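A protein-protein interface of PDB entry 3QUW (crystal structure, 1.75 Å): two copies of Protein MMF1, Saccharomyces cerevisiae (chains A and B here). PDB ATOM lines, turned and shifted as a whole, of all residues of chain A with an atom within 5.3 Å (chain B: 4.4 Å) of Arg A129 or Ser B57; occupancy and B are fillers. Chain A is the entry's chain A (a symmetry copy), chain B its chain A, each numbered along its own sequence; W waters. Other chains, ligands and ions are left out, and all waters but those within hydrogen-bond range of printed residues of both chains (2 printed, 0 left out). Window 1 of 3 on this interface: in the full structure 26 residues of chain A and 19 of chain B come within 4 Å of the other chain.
The backbone NH (N) of Gly B58 lies within hydrogen-bond range of the side-chain hydroxyl (OG) of Ser A130.
The side-chain hydroxyl of Ser B43 is in hydrogen-bond range of the guanidinium group of Arg A129.
The backbone NH of Gly B58 sits at hydrogen-bond distance from the backbone carbonyl oxygen of Arg A129, 3.3 Å away.
The backbone NH (N) of Ser B45 is in hydrogen-bond range of the backbone carbonyl oxygen (O) of Pro A127 (3.2 Å).
The side-chain hydroxyl of Ser B57 sits at hydrogen-bond distance from the backbone NH of Arg A129, 2.9 Å away.
The backbone carbonyl oxygen (O) of Ser A130 lies within hydrogen-bond range of the backbone NH (N) of Val A103 (2.9 Å).
N of Val A101 sits at hydrogen-bond distance from O of Ala A128.
The side-chain hydroxyl of Ser B57 lies within hydrogen-bond range of the backbone carbonyl oxygen of Ser B45 (2.7 Å).
The backbone carbonyl oxygen (O) of Gln B46 lies within hydrogen-bond range of the backbone NH (N) of Ser B57 (2.8 Å).
NE of Arg A129 is in hydrogen-bond range of SG of Cys A131 (3.5 Å).
NH1 of Arg A129 lies within hydrogen-bond range of OD1 of Asn A115, at 2.9 Å.
Lys A100 touches Tyr B55.
Ser B43 touches Asn A115 (OG to OD1, 3.98 Å).
OG of Ser B43 touches CD2 of Tyr A118 (3.6 Å).
Tyr B44 touches Pro A127 (CB to O, 3.4 Å).
CA of Ala A128 touches O of Ser B45, at 3.6 Å.
Ala A128 touches Tyr B55.
Ala A128 touches Ser B57 (CA to OG, 3.3 Å).
Arg A129 touches Tyr B44.
Of the printed residues of chain B, Lys A100 touches Tyr B55.
Phe A111 touches none of the printed residues of chain B.
Printed residues of chain B within 4 Å of Tyr A118: Ser B43 (3.6 Å).
Of the printed residues of chain B, Pro A127 touches Tyr B44 and Ser B45.
Arg A129 touches just these residues of chain B: Ser B43 (3.3 Å), Tyr B44 (3.4 Å), Ser B57 (2.9 Å) and Gly B58 (3.3 Å).
Of the printed residues of chain A, Tyr B44 touches Pro A127 and Arg A129.
Of the printed residues of chain A, Ser B45 touches Pro A127 and Ala A128.
Gln B46 touches none of the printed residues of chain A.
The nearest printed residue of chain B that does not touch Arg A129 is Ser B45 (4.5 Å).
The nearest printed residue of chain B that does not touch Ala A128 is Val B56 (4.4 Å).
Of the 10 printed residues of chain B, 6 touch a printed residue of chain A.
Printed residues of chain B that touch a printed residue of chain A: Ser B43, Tyr B44, Ser B45, Tyr B55, Ser B57 and Gly B58.
Hydrophobic or aromatic side chains of chain B that line the printed part of chain A: Tyr B44 and Tyr B55.
Hydrophobic or aromatic side chains of chain A within 4 Å of the printed part of chain B: Tyr A118 and Ala A128.
Among the printed residues, no Asp or Glu carboxylate lies within 4 Å of a Lys or Arg side-chain nitrogen of the other chain.
No position is printed for both chains.
Of the 13 pairs that touch across the chains among the printed residues, none has its exchanged pair printed and touching as well.
Water W1 lies within hydrogen-bond range of the backbone carbonyl oxygen of Ser B43, the side-chain hydroxyl of Tyr A118 and the backbone carbonyl oxygen of Pro A127.
Water W2 bridges NZ of Lys A100 (2.8 Å) and O of Val B56 (2.8 Å).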
ATOM      1  N   LYS A 100     -23.948  23.029 -17.379  1.00  0.00           N
ATOM      2  CA  LYS A 100     -23.379  22.056 -16.432  1.00  0.00           C
ATOM      3  C   LYS A 100     -24.398  21.768 -15.349  1.00  0.00           C
ATOM      4  O   LYS A 100     -25.017  22.684 -14.801  1.00  0.00           O
ATOM      5  CB  LYS A 100     -22.121  22.637 -15.798  1.00  0.00           C
ATOM      6  CG  LYS A 100     -21.536  21.808 -14.669  1.00  0.00           C
ATOM      7  CD  LYS A 100     -20.782  20.584 -15.212  1.00  0.00           C
ATOM      8  CE  LYS A 100     -20.212  19.707 -14.088  1.00  0.00           C
ATOM      9  NZ  LYS A 100     -19.293  20.462 -13.207  1.00  0.00           N
ATOM     10  N   VAL A 101     -24.535  20.487 -15.032  1.00  0.00           N
ATOM     11  CA  VAL A 101     -25.385  20.027 -13.949  1.00  0.00           C
ATOM     12  C   VAL A 101     -24.522  19.306 -12.910  1.00  0.00           C
ATOM     13  O   VAL A 101     -23.676  18.499 -13.276  1.00  0.00           O
ATOM     14  CB  VAL A 101     -26.438  19.032 -14.486  1.00  0.00           C
ATOM     15  CG1 VAL A 101     -27.330  18.555 -13.384  1.00  0.00           C
ATOM     16  CG2 VAL A 101     -27.254  19.676 -15.581  1.00  0.00           C
ATOM     17  N   VAL A 103     -25.167  16.846  -9.597  1.00  0.00           N
ATOM     18  CA  VAL A 103     -26.174  16.059  -8.883  1.00  0.00           C
ATOM     19  C   VAL A 103     -25.527  15.537  -7.611  1.00  0.00           C
ATOM     20  O   VAL A 103     -24.440  14.987  -7.664  1.00  0.00           O
ATOM     21  CB  VAL A 103     -26.657  14.871  -9.748  1.00  0.00           C
ATOM     22  CG1 VAL A 103     -27.679  14.002  -8.982  1.00  0.00           C
ATOM     23  CG2 VAL A 103     -27.252  15.382 -11.081  1.00  0.00           C
ATOM     24  N   PHE A 111     -29.050   6.094  -7.873  1.00  0.00           N
ATOM     25  CA  PHE A 111     -28.630   6.714  -9.110  1.00  0.00           C
ATOM     26  C   PHE A 111     -29.315   6.157 -10.358  1.00  0.00           C
ATOM     27  O   PHE A 111     -29.731   6.916 -11.212  1.00  0.00           O
ATOM     28  CB  PHE A 111     -27.124   6.637  -9.270  1.00  0.00           C
ATOM     29  CG  PHE A 111     -26.609   7.422 -10.440  1.00  0.00           C
ATOM     30  CD1 PHE A 111     -27.019   8.754 -10.643  1.00  0.00           C
ATOM     31  CD2 PHE A 111     -25.710   6.839 -11.332  1.00  0.00           C
ATOM     32  CE1 PHE A 111     -26.551   9.491 -11.736  1.00  0.00           C
ATOM     33  CE2 PHE A 111     -25.217   7.570 -12.427  1.00  0.00           C
ATOM     34  CZ  PHE A 111     -25.642   8.895 -12.635  1.00  0.00           C
ATOM     35  N   ASN A 115     -31.471   8.447 -12.822  1.00  0.00           N
ATOM     36  CA  ASN A 115     -31.009   8.602 -14.186  1.00  0.00           C
ATOM     37  C   ASN A 115     -32.122   8.425 -15.211  1.00  0.00           C
ATOM     38  O   ASN A 115     -32.128   9.092 -16.241  1.00  0.00           O
ATOM     39  CB  ASN A 115     -29.862   7.638 -14.487  1.00  0.00           C
ATOM     40  CG  ASN A 115     -29.114   8.021 -15.741  1.00  0.00           C
ATOM     41  OD1 ASN A 115     -28.334   8.983 -15.736  1.00  0.00           O
ATOM     42  ND2 ASN A 115     -29.358   7.287 -16.837  1.00  0.00           N
ATOM     43  N   TYR A 118     -33.686  11.781 -15.289  1.00  0.00           N
ATOM     44  CA  TYR A 118     -32.718  12.719 -15.863  1.00  0.00           C
ATOM     45  C   TYR A 118     -32.734  12.606 -17.385  1.00  0.00           C
ATOM     46  O   TYR A 118     -32.782  13.610 -18.094  1.00  0.00           O
ATOM     47  CB  TYR A 118     -31.318  12.418 -15.309  1.00  0.00           C
ATOM     48  CG  TYR A 118     -30.258  13.465 -15.612  1.00  0.00           C
ATOM     49  CD1 TYR A 118     -29.985  14.498 -14.706  1.00  0.00           C
ATOM     50  CD2 TYR A 118     -29.526  13.420 -16.787  1.00  0.00           C
ATOM     51  CE1 TYR A 118     -29.009  15.463 -14.978  1.00  0.00           C
ATOM     52  CE2 TYR A 118     -28.538  14.379 -17.069  1.00  0.00           C
ATOM     53  CZ  TYR A 118     -28.286  15.383 -16.147  1.00  0.00           C
ATOM     54  OH  TYR A 118     -27.341  16.320 -16.450  1.00  0.00           O
ATOM     55  N   PRO A 127     -26.021  18.644 -21.442  1.00  0.00           N
ATOM     56  CA  PRO A 127     -24.982  19.411 -20.743  1.00  0.00           C
ATOM     57  C   PRO A 127     -23.917  18.512 -20.119  1.00  0.00           C
ATOM     58  O   PRO A 127     -24.109  17.291 -19.967  1.00  0.00           O
ATOM     59  CB  PRO A 127     -25.744  20.159 -19.640  1.00  0.00           C
ATOM     60  CG  PRO A 127     -27.182  19.834 -19.810  1.00  0.00           C
ATOM     61  CD  PRO A 127     -27.327  18.704 -20.770  1.00  0.00           C
ATOM     62  N   ALA A 128     -22.800  19.113 -19.735  1.00  0.00           N
ATOM     63  CA  ALA A 128     -21.838  18.392 -18.930  1.00  0.00           C
ATOM     64  C   ALA A 128     -22.484  18.066 -17.572  1.00  0.00           C
ATOM     65  O   ALA A 128     -23.414  18.755 -17.151  1.00  0.00           O
ATOM     66  CB  ALA A 128     -20.614  19.234 -18.760  1.00  0.00           C
ATOM     67  N   ARG A 129     -21.987  17.026 -16.891  1.00  0.00           N
ATOM     68  CA  ARG A 129     -22.616  16.544 -15.648  1.00  0.00           C
ATOM     69  C   ARG A 129     -21.589  15.973 -14.693  1.00  0.00           C
ATOM     70  O   ARG A 129     -20.611  15.344 -15.132  1.00  0.00           O
ATOM     71  CB  ARG A 129     -23.650  15.470 -16.000  1.00  0.00           C
ATOM     72  CG  ARG A 129     -24.409  14.852 -14.834  1.00  0.00           C
ATOM     73  CD  ARG A 129     -25.402  13.796 -15.352  1.00  0.00           C
ATOM     74  NE  ARG A 129     -24.831  12.448 -15.480  1.00  0.00           N
ATOM     75  CZ  ARG A 129     -25.564  11.362 -15.737  1.00  0.00           C
ATOM     76  NH1 ARG A 129     -26.879  11.476 -15.887  1.00  0.00           N
ATOM     77  NH2 ARG A 129     -24.992  10.165 -15.815  1.00  0.00           N
ATOM     78  N   SER A 130     -21.802  16.178 -13.386  1.00  0.00           N
ATOM     79  CA  SER A 130     -21.062  15.429 -12.369  1.00  0.00           C
ATOM     80  C   SER A 130     -22.045  14.946 -11.336  1.00  0.00           C
ATOM     81  O   SER A 130     -22.974  15.664 -10.993  1.00  0.00           O
ATOM     82  CB  SER A 130     -20.003  16.284 -11.672  1.00  0.00           C
ATOM     83  OG  SER A 130     -19.008  16.744 -12.590  1.00  0.00           O
ATOM     84  N   CYS A 131     -21.817  13.750 -10.816  1.00  0.00           N
ATOM     85  CA  CYS A 131     -22.742  13.135  -9.865  1.00  0.00           C
ATOM     86  C   CYS A 131     -21.916  12.555  -8.744  1.00  0.00           C
ATOM     87  O   CYS A 131     -20.956  11.833  -9.001  1.00  0.00           O
ATOM     88  CB  CYS A 131     -23.523  12.012 -10.541  1.00  0.00           C
ATOM     89  SG  CYS A 131     -24.481  12.529 -11.961  1.00  0.00           S
ATOM     90  N   SER B  43     -27.462  10.748 -21.858  1.00  0.00           N
ATOM     91  CA  SER B  43     -28.053  11.966 -21.293  1.00  0.00           C
ATOM     92  C   SER B  43     -27.080  13.146 -21.052  1.00  0.00           C
ATOM     93  O   SER B  43     -27.520  14.221 -20.622  1.00  0.00           O
ATOM     94  CB  SER B  43     -28.770  11.627 -19.988  1.00  0.00           C
ATOM     95  OG  SER B  43     -27.836  11.165 -19.027  1.00  0.00           O
ATOM     96  N   TYR B  44     -25.779  12.959 -21.304  1.00  0.00           N
ATOM     97  CA  TYR B  44     -24.796  14.035 -21.032  1.00  0.00           C
ATOM     98  C   TYR B  44     -23.641  14.074 -22.051  1.00  0.00           C
ATOM     99  O   TYR B  44     -23.527  13.189 -22.905  1.00  0.00           O
ATOM    100  CB  TYR B  44     -24.268  13.947 -19.589  1.00  0.00           C
ATOM    101  CG  TYR B  44     -23.398  12.740 -19.281  1.00  0.00           C
ATOM    102  CD1 TYR B  44     -22.002  12.827 -19.322  1.00  0.00           C
ATOM    103  CD2 TYR B  44     -23.973  11.518 -18.934  1.00  0.00           C
ATOM    104  CE1 TYR B  44     -21.209  11.711 -19.039  1.00  0.00           C
ATOM    105  CE2 TYR B  44     -23.197  10.411 -18.642  1.00  0.00           C
ATOM    106  CZ  TYR B  44     -21.823  10.506 -18.708  1.00  0.00           C
ATOM    107  OH  TYR B  44     -21.077   9.376 -18.432  1.00  0.00           O
ATOM    108  N   SER B  45     -22.803  15.102 -21.967  1.00  0.00           N
ATOM    109  CA  SER B  45     -21.658  15.235 -22.857  1.00  0.00           C
ATOM    110  C   SER B  45     -20.382  15.260 -22.033  1.00  0.00           C
ATOM    111  O   SER B  45     -20.373  15.722 -20.890  1.00  0.00           O
ATOM    112  CB  SER B  45     -21.762  16.520 -23.679  1.00  0.00           C
ATOM    113  OG  SER B  45     -22.910  16.500 -24.524  1.00  0.00           O
ATOM    114  N   GLN B  46     -19.289  14.782 -22.614  1.00  0.00           N
ATOM    115  CA  GLN B  46     -18.006  14.789 -21.895  1.00  0.00           C
ATOM    116  C   GLN B  46     -17.629  16.201 -21.481  1.00  0.00           C
ATOM    117  O   GLN B  46     -17.085  16.411 -20.411  1.00  0.00           O
ATOM    118  CB  GLN B  46     -16.905  14.199 -22.772  1.00  0.00           C
ATOM    119  CG  GLN B  46     -17.017  12.709 -22.971  1.00  0.00           C
ATOM    120  CD  GLN B  46     -16.117  12.254 -24.092  1.00  0.00           C
ATOM    121  OE1 GLN B  46     -15.813  13.031 -24.998  1.00  0.00           O
ATOM    122  NE2 GLN B  46     -15.655  11.016 -24.025  1.00  0.00           N
ATOM    123  N   TYR B  55     -16.754  23.462 -19.710  1.00  0.00           N
ATOM    124  CA  TYR B  55     -17.159  22.703 -18.512  1.00  0.00           C
ATOM    125  C   TYR B  55     -17.014  21.221 -18.796  1.00  0.00           C
ATOM    126  O   TYR B  55     -17.714  20.683 -19.668  1.00  0.00           O
ATOM    127  CB  TYR B  55     -18.602  23.006 -18.128  1.00  0.00           C
ATOM    128  CG  TYR B  55     -18.794  24.361 -17.486  1.00  0.00           C
ATOM    129  CD1 TYR B  55     -18.841  24.485 -16.104  1.00  0.00           C
ATOM    130  CD2 TYR B  55     -18.924  25.513 -18.259  1.00  0.00           C
ATOM    131  CE1 TYR B  55     -19.025  25.709 -15.494  1.00  0.00           C
ATOM    132  CE2 TYR B  55     -19.110  26.775 -17.640  1.00  0.00           C
ATOM    133  CZ  TYR B  55     -19.156  26.847 -16.257  1.00  0.00           C
ATOM    134  OH  TYR B  55     -19.335  28.064 -15.607  1.00  0.00           O
ATOM    135  N   VAL B  56     -16.078  20.582 -18.089  1.00  0.00           N
ATOM    136  CA  VAL B  56     -15.778  19.168 -18.306  1.00  0.00           C
ATOM    137  C   VAL B  56     -16.521  18.343 -17.260  1.00  0.00           C
ATOM    138  O   VAL B  56     -16.473  18.652 -16.070  1.00  0.00           O
ATOM    139  CB  VAL B  56     -14.256  18.908 -18.237  1.00  0.00           C
ATOM    140  CG1 VAL B  56     -13.937  17.454 -18.419  1.00  0.00           C
ATOM    141  CG2 VAL B  56     -13.552  19.726 -19.309  1.00  0.00           C
ATOM    142  N   SER B  57     -17.228  17.318 -17.719  1.00  0.00           N
ATOM    143  CA  SER B  57     -17.900  16.378 -16.824  1.00  0.00           C
ATOM    144  C   SER B  57     -16.894  15.702 -15.899  1.00  0.00           C
ATOM    145  O   SER B  57     -15.729  15.519 -16.257  1.00  0.00           O
ATOM    146  CB  SER B  57     -18.628  15.317 -17.640  1.00  0.00           C
ATOM    147  OG  SER B  57     -19.704  15.902 -18.326  1.00  0.00           O
ATOM    148  N   GLY B  58     -17.347  15.334 -14.710  1.00  0.00           N
ATOM    149  CA  GLY B  58     -16.485  14.619 -13.757  1.00  0.00           C
ATOM    150  C   GLY B  58     -15.957  13.342 -14.377  1.00  0.00           C
ATOM    151  O   GLY B  58     -16.728  12.462 -14.807  1.00  0.00           O
ATOM    152  N   GLN B  59     -14.633  13.265 -14.454  1.00  0.00           N
ATOM    153  CA  GLN B  59     -13.942  12.129 -15.030  1.00  0.00           C
ATOM    154  C   GLN B  59     -13.559  11.143 -13.943  1.00  0.00           C
ATOM    155  O   GLN B  59     -13.166  11.542 -12.856  1.00  0.00           O
ATOM    156  CB  GLN B  59     -12.698  12.569 -15.804  1.00  0.00           C
ATOM    157  CG  GLN B  59     -13.059  13.398 -17.041  1.00  0.00           C
ATOM    158  CD  GLN B  59     -14.004  12.662 -17.951  1.00  0.00           C
ATOM    159  OE1 GLN B  59     -13.657  11.645 -18.546  1.00  0.00           O
ATOM    160  NE2 GLN B  59     -15.218  13.181 -18.076  1.00  0.00           N
ATOM    161  N   MET B 145     -12.946  13.726 -10.894  1.00  0.00           N
ATOM    162  CA  MET B 145     -12.410  15.086 -10.999  1.00  0.00           C
ATOM    163  C   MET B 145     -13.096  15.842 -12.123  1.00  0.00           C
ATOM    164  O   MET B 145     -13.154  15.354 -13.251  1.00  0.00           O
ATOM    165  CB  MET B 145     -10.892  15.036 -11.207  1.00  0.00           C
ATOM    166  CG  MET B 145     -10.220  16.424 -11.208  1.00  0.00           C
ATOM    167  SD  MET B 145      -8.408  16.316 -11.235  1.00  0.00           S
ATOM    168  CE  MET B 145      -8.138  15.952 -12.969  1.00  0.00           C
HETATM  169  O   HOH W   1     -26.673  16.179 -19.035  1.00  0.00           O
HETATM  170  O   HOH W   2     -17.218  21.154 -14.954  1.00  0.00           O
